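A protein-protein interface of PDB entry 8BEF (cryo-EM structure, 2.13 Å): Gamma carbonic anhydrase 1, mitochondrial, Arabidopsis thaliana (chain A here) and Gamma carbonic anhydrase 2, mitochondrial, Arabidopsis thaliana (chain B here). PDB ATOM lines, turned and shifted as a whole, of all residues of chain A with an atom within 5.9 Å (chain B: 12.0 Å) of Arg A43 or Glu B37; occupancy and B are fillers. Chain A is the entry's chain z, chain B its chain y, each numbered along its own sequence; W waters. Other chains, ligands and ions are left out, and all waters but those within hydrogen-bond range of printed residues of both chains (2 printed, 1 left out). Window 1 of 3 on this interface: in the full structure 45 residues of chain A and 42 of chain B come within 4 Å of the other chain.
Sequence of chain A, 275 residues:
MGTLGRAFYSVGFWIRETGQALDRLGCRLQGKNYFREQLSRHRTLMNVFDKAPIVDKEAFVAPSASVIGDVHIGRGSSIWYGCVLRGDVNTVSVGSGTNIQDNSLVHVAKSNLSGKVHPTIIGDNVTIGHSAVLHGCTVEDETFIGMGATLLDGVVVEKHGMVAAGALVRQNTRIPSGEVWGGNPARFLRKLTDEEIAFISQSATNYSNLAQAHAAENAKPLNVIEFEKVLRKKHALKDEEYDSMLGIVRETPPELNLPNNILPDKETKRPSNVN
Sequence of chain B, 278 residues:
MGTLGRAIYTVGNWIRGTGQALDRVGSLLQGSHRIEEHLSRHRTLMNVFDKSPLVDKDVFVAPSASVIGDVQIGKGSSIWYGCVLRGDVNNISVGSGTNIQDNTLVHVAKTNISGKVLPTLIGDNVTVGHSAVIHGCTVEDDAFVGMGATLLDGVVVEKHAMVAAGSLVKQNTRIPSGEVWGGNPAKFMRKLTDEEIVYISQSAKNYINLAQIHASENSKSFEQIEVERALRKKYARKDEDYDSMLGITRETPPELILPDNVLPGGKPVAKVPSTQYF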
ATOM      1  N   LEU A  39      -5.396 -10.926   4.598  1.00  0.00           N
ATOM      2  CA  LEU A  39      -4.331 -11.886   4.836  1.00  0.00           C
ATOM      3  C   LEU A  39      -2.995 -11.246   4.485  1.00  0.00           C
ATOM      4  O   LEU A  39      -2.903 -10.455   3.543  1.00  0.00           O
ATOM      5  CB  LEU A  39      -4.540 -13.168   4.025  1.00  0.00           C
ATOM      6  CG  LEU A  39      -5.866 -13.904   4.242  1.00  0.00           C
ATOM      7  CD1 LEU A  39      -6.380 -14.504   2.935  1.00  0.00           C
ATOM      8  CD2 LEU A  39      -5.776 -14.958   5.341  1.00  0.00           C
ATOM      9  N   SER A  40      -1.966 -11.584   5.256  1.00  0.00           N
ATOM     10  CA  SER A  40      -0.675 -10.928   5.105  1.00  0.00           C
ATOM     11  C   SER A  40      -0.089 -11.196   3.725  1.00  0.00           C
ATOM     12  O   SER A  40      -0.061 -12.335   3.255  1.00  0.00           O
ATOM     13  CB  SER A  40       0.292 -11.403   6.184  1.00  0.00           C
ATOM     14  OG  SER A  40       1.598 -10.917   5.933  1.00  0.00           O
ATOM     15  N   ARG A  41       0.392 -10.137   3.086  1.00  0.00           N
ATOM     16  CA  ARG A  41       1.042 -10.232   1.790  1.00  0.00           C
ATOM     17  C   ARG A  41       2.559 -10.262   1.911  1.00  0.00           C
ATOM     18  O   ARG A  41       3.258 -10.083   0.911  1.00  0.00           O
ATOM     19  CB  ARG A  41       0.583  -9.080   0.896  1.00  0.00           C
ATOM     20  CG  ARG A  41      -0.930  -8.883   0.937  1.00  0.00           C
ATOM     21  CD  ARG A  41      -1.444  -7.992  -0.180  1.00  0.00           C
ATOM     22  NE  ARG A  41      -1.143  -8.516  -1.507  1.00  0.00           N
ATOM     23  CZ  ARG A  41      -1.620  -8.004  -2.635  1.00  0.00           C
ATOM     24  NH1 ARG A  41      -2.437  -6.964  -2.629  1.00  0.00           N
ATOM     25  NH2 ARG A  41      -1.266  -8.546  -3.796  1.00  0.00           N
ATOM     26  N   HIS A  42       3.076 -10.473   3.118  1.00  0.00           N
ATOM     27  CA  HIS A  42       4.512 -10.577   3.316  1.00  0.00           C
ATOM     28  C   HIS A  42       5.071 -11.773   2.560  1.00  0.00           C
ATOM     29  O   HIS A  42       4.525 -12.875   2.623  1.00  0.00           O
ATOM     30  CB  HIS A  42       4.837 -10.709   4.802  1.00  0.00           C
ATOM     31  CG  HIS A  42       6.240 -11.158   5.065  1.00  0.00           C
ATOM     32  ND1 HIS A  42       7.328 -10.330   4.895  1.00  0.00           N
ATOM     33  CD2 HIS A  42       6.736 -12.351   5.472  1.00  0.00           C
ATOM     34  CE1 HIS A  42       8.432 -10.989   5.194  1.00  0.00           C
ATOM     35  NE2 HIS A  42       8.101 -12.219   5.546  1.00  0.00           N
ATOM     36  N   ARG A  43       6.171 -11.548   1.853  1.00  0.00           N
ATOM     37  CA  ARG A  43       6.916 -12.605   1.190  1.00  0.00           C
ATOM     38  C   ARG A  43       8.319 -12.638   1.776  1.00  0.00           C
ATOM     39  O   ARG A  43       8.997 -11.607   1.825  1.00  0.00           O
ATOM     40  CB  ARG A  43       6.964 -12.380  -0.325  1.00  0.00           C
ATOM     41  CG  ARG A  43       5.701 -12.825  -1.055  1.00  0.00           C
ATOM     42  CD  ARG A  43       5.728 -12.439  -2.527  1.00  0.00           C
ATOM     43  NE  ARG A  43       5.689 -10.995  -2.716  1.00  0.00           N
ATOM     44  CZ  ARG A  43       6.034 -10.370  -3.832  1.00  0.00           C
ATOM     45  NH1 ARG A  43       6.441 -11.034  -4.902  1.00  0.00           N
ATOM     46  NH2 ARG A  43       5.958  -9.043  -3.882  1.00  0.00           N
ATOM     47  N   THR A  44       8.744 -13.814   2.235  1.00  0.00           N
ATOM     48  CA  THR A  44      10.091 -13.946   2.780  1.00  0.00           C
ATOM     49  C   THR A  44      11.138 -13.611   1.726  1.00  0.00           C
ATOM     50  O   THR A  44      12.113 -12.907   2.008  1.00  0.00           O
ATOM     51  CB  THR A  44      10.300 -15.360   3.323  1.00  0.00           C
ATOM     52  OG1 THR A  44       9.262 -15.672   4.260  1.00  0.00           O
ATOM     53  CG2 THR A  44      11.643 -15.474   4.011  1.00  0.00           C
ATOM     54  N   LEU A  45      10.944 -14.099   0.507  1.00  0.00           N
ATOM     55  CA  LEU A  45      11.754 -13.721  -0.640  1.00  0.00           C
ATOM     56  C   LEU A  45      10.886 -12.930  -1.605  1.00  0.00           C
ATOM     57  O   LEU A  45       9.824 -13.405  -2.019  1.00  0.00           O
ATOM     58  CB  LEU A  45      12.337 -14.952  -1.334  1.00  0.00           C
ATOM     59  CG  LEU A  45      13.032 -15.980  -0.439  1.00  0.00           C
ATOM     60  CD1 LEU A  45      13.593 -17.116  -1.280  1.00  0.00           C
ATOM     61  CD2 LEU A  45      14.129 -15.328   0.397  1.00  0.00           C
ATOM     62  N   MET A  46      11.338 -11.734  -1.964  1.00  0.00           N
ATOM     63  CA  MET A  46      10.580 -10.845  -2.832  1.00  0.00           C
ATOM     64  C   MET A  46      11.436 -10.423  -4.013  1.00  0.00           C
ATOM     65  O   MET A  46      12.573  -9.977  -3.835  1.00  0.00           O
ATOM     66  CB  MET A  46      10.093  -9.605  -2.078  1.00  0.00           C
ATOM     67  CG  MET A  46       9.083  -8.789  -2.860  1.00  0.00           C
ATOM     68  SD  MET A  46       8.463  -7.350  -1.972  1.00  0.00           S
ATOM     69  CE  MET A  46       8.130  -6.240  -3.339  1.00  0.00           C
ATOM     70  N   ASN A  47      10.875 -10.539  -5.210  1.00  0.00           N
ATOM     71  CA  ASN A  47      11.529 -10.080  -6.420  1.00  0.00           C
ATOM     72  C   ASN A  47      11.094  -8.659  -6.754  1.00  0.00           C
ATOM     73  O   ASN A  47       9.971  -8.241  -6.462  1.00  0.00           O
ATOM     74  CB  ASN A  47      11.202 -11.005  -7.593  1.00  0.00           C
ATOM     75  CG  ASN A  47       9.747 -10.920  -8.009  1.00  0.00           C
ATOM     76  OD1 ASN A  47       8.878 -11.516  -7.379  1.00  0.00           O
ATOM     77  ND2 ASN A  47       9.477 -10.168  -9.067  1.00  0.00           N
ATOM     78  N   PRO A  63      10.949 -17.148   8.600  1.00  0.00           N
ATOM     79  CA  PRO A  63       9.818 -16.743   7.744  1.00  0.00           C
ATOM     80  C   PRO A  63       9.510 -15.257   7.801  1.00  0.00           C
ATOM     81  O   PRO A  63       9.130 -14.670   6.781  1.00  0.00           O
ATOM     82  CB  PRO A  63       8.652 -17.585   8.286  1.00  0.00           C
ATOM     83  CG  PRO A  63       9.296 -18.747   8.966  1.00  0.00           C
ATOM     84  CD  PRO A  63      10.599 -18.246   9.517  1.00  0.00           C
ATOM     85  N   ALA A  65      11.586 -12.845   8.105  1.00  0.00           N
ATOM     86  CA  ALA A  65      12.621 -12.022   7.497  1.00  0.00           C
ATOM     87  C   ALA A  65      12.185 -11.533   6.119  1.00  0.00           C
ATOM     88  O   ALA A  65      11.383 -12.171   5.433  1.00  0.00           O
ATOM     89  CB  ALA A  65      13.927 -12.805   7.383  1.00  0.00           C
ATOM     90  N   SER A  66      12.720 -10.383   5.718  1.00  0.00           N
ATOM     91  CA  SER A  66      12.456  -9.796   4.410  1.00  0.00           C
ATOM     92  C   SER A  66      13.741  -9.802   3.591  1.00  0.00           C
ATOM     93  O   SER A  66      14.713  -9.130   3.947  1.00  0.00           O
ATOM     94  CB  SER A  66      11.915  -8.371   4.540  1.00  0.00           C
ATOM     95  OG  SER A  66      10.732  -8.328   5.312  1.00  0.00           O
ATOM     96  N   VAL A  67      13.740 -10.559   2.500  1.00  0.00           N
ATOM     97  CA  VAL A  67      14.836 -10.580   1.540  1.00  0.00           C
ATOM     98  C   VAL A  67      14.274 -10.062   0.223  1.00  0.00           C
ATOM     99  O   VAL A  67      13.421 -10.714  -0.392  1.00  0.00           O
ATOM    100  CB  VAL A  67      15.433 -11.985   1.381  1.00  0.00           C
ATOM    101  CG1 VAL A  67      16.670 -11.942   0.529  1.00  0.00           C
ATOM    102  CG2 VAL A  67      15.738 -12.595   2.751  1.00  0.00           C
ATOM    103  N   ASP B  23      -5.322 -16.028 -14.979  1.00  0.00           N
ATOM    104  CA  ASP B  23      -4.242 -15.692 -14.056  1.00  0.00           C
ATOM    105  C   ASP B  23      -2.991 -16.512 -14.353  1.00  0.00           C
ATOM    106  O   ASP B  23      -1.874 -15.981 -14.338  1.00  0.00           O
ATOM    107  CB  ASP B  23      -4.698 -15.898 -12.610  1.00  0.00           C
ATOM    108  CG  ASP B  23      -3.793 -15.205 -11.601  1.00  0.00           C
ATOM    109  OD1 ASP B  23      -3.178 -14.177 -11.944  1.00  0.00           O
ATOM    110  OD2 ASP B  23      -3.695 -15.691 -10.456  1.00  0.00           O
ATOM    111  N   SER B  27       0.639 -15.104 -15.526  1.00  0.00           N
ATOM    112  CA  SER B  27       1.873 -15.466 -14.838  1.00  0.00           C
ATOM    113  C   SER B  27       2.915 -15.993 -15.818  1.00  0.00           C
ATOM    114  O   SER B  27       4.101 -15.669 -15.705  1.00  0.00           O
ATOM    115  CB  SER B  27       1.586 -16.498 -13.750  1.00  0.00           C
ATOM    116  OG  SER B  27       0.682 -15.985 -12.789  1.00  0.00           O
ATOM    117  N   GLN B  30       4.648 -13.223 -17.669  1.00  0.00           N
ATOM    118  CA  GLN B  30       5.610 -12.447 -16.840  1.00  0.00           C
ATOM    119  C   GLN B  30       6.933 -13.213 -16.713  1.00  0.00           C
ATOM    120  O   GLN B  30       7.783 -12.800 -15.951  1.00  0.00           O
ATOM    121  CB  GLN B  30       5.035 -12.192 -15.447  1.00  0.00           C
ATOM    122  CG  GLN B  30       3.817 -11.302 -15.356  1.00  0.00           C
ATOM    123  CD  GLN B  30       3.508 -11.002 -13.909  1.00  0.00           C
ATOM    124  OE1 GLN B  30       3.526 -11.876 -13.054  1.00  0.00           O
ATOM    125  NE2 GLN B  30       3.256  -9.740 -13.621  1.00  0.00           N
ATOM    126  N   SER B  32       7.353 -15.979 -15.320  1.00  0.00           N
ATOM    127  CA  SER B  32       7.322 -16.672 -14.034  1.00  0.00           C
ATOM    128  C   SER B  32       8.269 -16.050 -13.015  1.00  0.00           C
ATOM    129  O   SER B  32       8.710 -16.723 -12.081  1.00  0.00           O
ATOM    130  CB  SER B  32       7.631 -18.161 -14.203  1.00  0.00           C
ATOM    131  OG  SER B  32       6.457 -18.888 -14.514  1.00  0.00           O
ATOM    132  N   HIS B  33       8.591 -14.766 -13.176  1.00  0.00           N
ATOM    133  CA  HIS B  33       9.556 -14.122 -12.295  1.00  0.00           C
ATOM    134  C   HIS B  33       8.964 -13.786 -10.933  1.00  0.00           C
ATOM    135  O   HIS B  33       9.688 -13.800  -9.932  1.00  0.00           O
ATOM    136  CB  HIS B  33      10.101 -12.853 -12.949  1.00  0.00           C
ATOM    137  CG  HIS B  33      11.093 -13.117 -14.035  1.00  0.00           C
ATOM    138  ND1 HIS B  33      11.705 -14.340 -14.200  1.00  0.00           N
ATOM    139  CD2 HIS B  33      11.579 -12.317 -15.012  1.00  0.00           C
ATOM    140  CE1 HIS B  33      12.524 -14.282 -15.234  1.00  0.00           C
ATOM    141  NE2 HIS B  33      12.469 -13.066 -15.743  1.00  0.00           N
ATOM    142  N   ARG B  34       7.655 -13.556 -10.880  1.00  0.00           N
ATOM    143  CA  ARG B  34       6.988 -13.116  -9.641  1.00  0.00           C
ATOM    144  C   ARG B  34       6.915 -14.239  -8.633  1.00  0.00           C
ATOM    145  O   ARG B  34       6.175 -15.174  -8.891  1.00  0.00           O
ATOM    146  CB  ARG B  34       5.646 -12.440  -9.925  1.00  0.00           C
ATOM    147  CG  ARG B  34       5.181 -11.655  -8.707  1.00  0.00           C
ATOM    148  CD  ARG B  34       3.754 -11.157  -8.738  1.00  0.00           C
ATOM    149  NE  ARG B  34       3.419 -10.308  -7.601  1.00  0.00           N
ATOM    150  CZ  ARG B  34       2.866 -10.725  -6.471  1.00  0.00           C
ATOM    151  NH1 ARG B  34       2.583 -12.003  -6.300  1.00  0.00           N
ATOM    152  NH2 ARG B  34       2.624  -9.866  -5.500  1.00  0.00           N
ATOM    153  N   ILE B  35       7.618 -14.089  -7.511  1.00  0.00           N
ATOM    154  CA  ILE B  35       7.444 -15.061  -6.442  1.00  0.00           C
ATOM    155  C   ILE B  35       6.038 -14.920  -5.875  1.00  0.00           C
ATOM    156  O   ILE B  35       5.585 -13.813  -5.560  1.00  0.00           O
ATOM    157  CB  ILE B  35       8.517 -14.866  -5.361  1.00  0.00           C
ATOM    158  CG1 ILE B  35       9.909 -15.154  -5.935  1.00  0.00           C
ATOM    159  CG2 ILE B  35       8.233 -15.748  -4.160  1.00  0.00           C
ATOM    160  CD1 ILE B  35      11.042 -14.721  -5.046  1.00  0.00           C
ATOM    161  N   GLU B  36       5.337 -16.041  -5.747  1.00  0.00           N
ATOM    162  CA  GLU B  36       3.943 -16.010  -5.327  1.00  0.00           C
ATOM    163  C   GLU B  36       3.816 -15.807  -3.823  1.00  0.00           C
ATOM    164  O   GLU B  36       4.587 -16.358  -3.034  1.00  0.00           O
ATOM    165  CB  GLU B  36       3.234 -17.300  -5.732  1.00  0.00           C
ATOM    166  CG  GLU B  36       3.125 -17.498  -7.226  1.00  0.00           C
ATOM    167  CD  GLU B  36       1.866 -18.245  -7.618  1.00  0.00           C
ATOM    168  OE1 GLU B  36       1.639 -19.350  -7.083  1.00  0.00           O
ATOM    169  OE2 GLU B  36       1.100 -17.725  -8.456  1.00  0.00           O
ATOM    170  N   GLU B  37       2.836 -14.998  -3.436  1.00  0.00           N
ATOM    171  CA  GLU B  37       2.447 -14.897  -2.040  1.00  0.00           C
ATOM    172  C   GLU B  37       1.869 -16.229  -1.571  1.00  0.00           C
ATOM    173  O   GLU B  37       1.252 -16.967  -2.341  1.00  0.00           O
ATOM    174  CB  GLU B  37       1.429 -13.770  -1.871  1.00  0.00           C
ATOM    175  CG  GLU B  37       1.937 -12.406  -2.323  1.00  0.00           C
ATOM    176  CD  GLU B  37       0.855 -11.355  -2.321  1.00  0.00           C
ATOM    177  OE1 GLU B  37       0.633 -10.726  -3.372  1.00  0.00           O
ATOM    178  OE2 GLU B  37       0.197 -11.184  -1.276  1.00  0.00           O
ATOM    179  N   HIS B  38       2.075 -16.544  -0.294  1.00  0.00           N
ATOM    180  CA  HIS B  38       1.675 -17.840   0.235  1.00  0.00           C
ATOM    181  C   HIS B  38       1.059 -17.679   1.618  1.00  0.00           C
ATOM    182  O   HIS B  38       1.054 -16.594   2.203  1.00  0.00           O
ATOM    183  CB  HIS B  38       2.859 -18.813   0.289  1.00  0.00           C
ATOM    184  CG  HIS B  38       3.437 -19.134  -1.052  1.00  0.00           C
ATOM    185  ND1 HIS B  38       2.680 -19.645  -2.085  1.00  0.00           N
ATOM    186  CD2 HIS B  38       4.698 -19.018  -1.531  1.00  0.00           C
ATOM    187  CE1 HIS B  38       3.450 -19.825  -3.144  1.00  0.00           C
ATOM    188  NE2 HIS B  38       4.679 -19.454  -2.834  1.00  0.00           N
ATOM    189  N   LEU B  39       0.528 -18.787   2.130  1.00  0.00           N
ATOM    190  CA  LEU B  39       0.004 -18.823   3.487  1.00  0.00           C
ATOM    191  C   LEU B  39       1.097 -18.465   4.486  1.00  0.00           C
ATOM    192  O   LEU B  39       2.250 -18.878   4.342  1.00  0.00           O
ATOM    193  CB  LEU B  39      -0.551 -20.212   3.793  1.00  0.00           C
ATOM    194  CG  LEU B  39      -1.674 -20.310   4.819  1.00  0.00           C
ATOM    195  CD1 LEU B  39      -2.806 -19.362   4.472  1.00  0.00           C
ATOM    196  CD2 LEU B  39      -2.165 -21.737   4.915  1.00  0.00           C
ATOM    197  N   SER B  40       0.730 -17.690   5.504  1.00  0.00           N
ATOM    198  CA  SER B  40       1.713 -17.218   6.468  1.00  0.00           C
ATOM    199  C   SER B  40       2.284 -18.382   7.268  1.00  0.00           C
ATOM    200  O   SER B  40       1.540 -19.189   7.834  1.00  0.00           O
ATOM    201  CB  SER B  40       1.092 -16.186   7.408  1.00  0.00           C
ATOM    202  OG  SER B  40       2.035 -15.742   8.366  1.00  0.00           O
ATOM    203  N   ARG B  41       3.609 -18.462   7.319  1.00  0.00           N
ATOM    204  CA  ARG B  41       4.307 -19.497   8.065  1.00  0.00           C
ATOM    205  C   ARG B  41       4.892 -18.990   9.376  1.00  0.00           C
ATOM    206  O   ARG B  41       5.555 -19.758  10.079  1.00  0.00           O
ATOM    207  CB  ARG B  41       5.415 -20.110   7.201  1.00  0.00           C
ATOM    208  CG  ARG B  41       4.893 -20.864   5.982  1.00  0.00           C
ATOM    209  CD  ARG B  41       5.920 -21.839   5.433  1.00  0.00           C
ATOM    210  NE  ARG B  41       6.294 -22.853   6.411  1.00  0.00           N
ATOM    211  CZ  ARG B  41       5.788 -24.077   6.455  1.00  0.00           C
ATOM    212  NH1 ARG B  41       4.880 -24.481   5.583  1.00  0.00           N
ATOM    213  NH2 ARG B  41       6.200 -24.915   7.401  1.00  0.00           N
ATOM    214  N   HIS B  42       4.671 -17.726   9.719  1.00  0.00           N
ATOM    215  CA  HIS B  42       5.193 -17.192  10.970  1.00  0.00           C
ATOM    216  C   HIS B  42       4.428 -17.769  12.152  1.00  0.00           C
ATOM    217  O   HIS B  42       3.194 -17.767  12.168  1.00  0.00           O
ATOM    218  CB  HIS B  42       5.100 -15.670  10.983  1.00  0.00           C
ATOM    219  CG  HIS B  42       5.317 -15.070  12.337  1.00  0.00           C
ATOM    220  ND1 HIS B  42       6.559 -15.000  12.930  1.00  0.00           N
ATOM    221  CD2 HIS B  42       4.447 -14.527  13.221  1.00  0.00           C
ATOM    222  CE1 HIS B  42       6.446 -14.429  14.116  1.00  0.00           C
ATOM    223  NE2 HIS B  42       5.175 -14.133  14.317  1.00  0.00           N
HETATM  224  O   HOH W   1       0.591 -14.726   4.339  1.00  0.00           O
HETATM  225  O   HOH W   2      -0.106  -8.856  -6.966  1.00  0.00           O
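The backbone carbonyl oxygen (O) of Ile B35 lies within hydrogen-bond range of the guanidinium group (NH1) of Arg A43 (3.0 Å).
The backbone NH (N) of Ile B35 sits at hydrogen-bond distance from the side-chain amide oxygen (OD1) of Asn A47 (2.9 Å).
The side-chain carboxylate of Glu B37 lies within salt-bridge range of the guanidinium group of Arg A41 (2.9 Å).
The side-chain carboxylate of Glu B37 is in salt-bridge range of the guanidinium group of Arg B34, 3.0 Å away.
NH2 of Arg A43 sits close to SD of Met A46 (3.6 Å).
Among the printed residues, pairs that only touch across the chains: Asn A47 with Arg B34, Asn A47 with His B33, Leu A45 with Ile B35, Arg A43 with Arg B34 and Arg A43 with Glu B37.
Of chain B, only Arg B34, Ile B35 and Glu B37 come within 4 Å of Arg A43.
Glu B37 touches just these residues of chain A: Arg A41 and Arg A43.
Of chain B, only Glu B37 (2.9 Å) comes within 4 Å of Arg A41.
No residue of chain B comes within 4 Å of His A42.
Met A46 touches none of the printed residues of chain B.
Asn A47 touches just these residues of chain B: His B33, Arg B34 and Ile B35.
No residue of chain B comes within 4 Å of Ser A66.
No residue of chain B comes within 4 Å of Val A67.
Of the printed residues of chain A, Ile B35 touches Arg A43 (3.0 Å), Leu A45 (3.5 Å) and Asn A47 (2.9 Å).
Of the printed residues of chain A, His B33 touches Asn A47 (3.5 Å).
Of the printed residues of chain A, Arg B34 touches Arg A43 (3.8 Å) and Asn A47 (3.4 Å).
Ser B40 touches none of the printed residues of chain A.
Leu A39 touches none of the printed residues of chain B.
Of the 13 printed residues of chain A, 4 touch a printed residue of chain B.
Printed residues of chain A that touch a printed residue of chain B: Arg A41, Arg A43, Leu A45 and Asn A47.
Hydrophobic or aromatic side chains of chain A within 4 Å of the printed part of chain B: Leu A45.
Of the 14 printed residues of chain B, 4 touch a printed residue of chain A.
Printed residues of chain B that touch a printed residue of chain A: His B33, Arg B34, Ile B35 and Glu B37.
Among the printed residues, Asp or Glu carboxylates within 4 Å of a Lys or Arg side-chain nitrogen of the other chain: Arg A41 with Glu B37.
Water W1 lies within hydrogen-bond range of O of Ser A40 (2.7 Å), O of His B38 (2.9 Å) and N of Ser B40 (3.2 Å).
Water W2 bridges the guanidinium group (NH2) of Arg B34 and the guanidinium group (NH2) of Arg A41.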
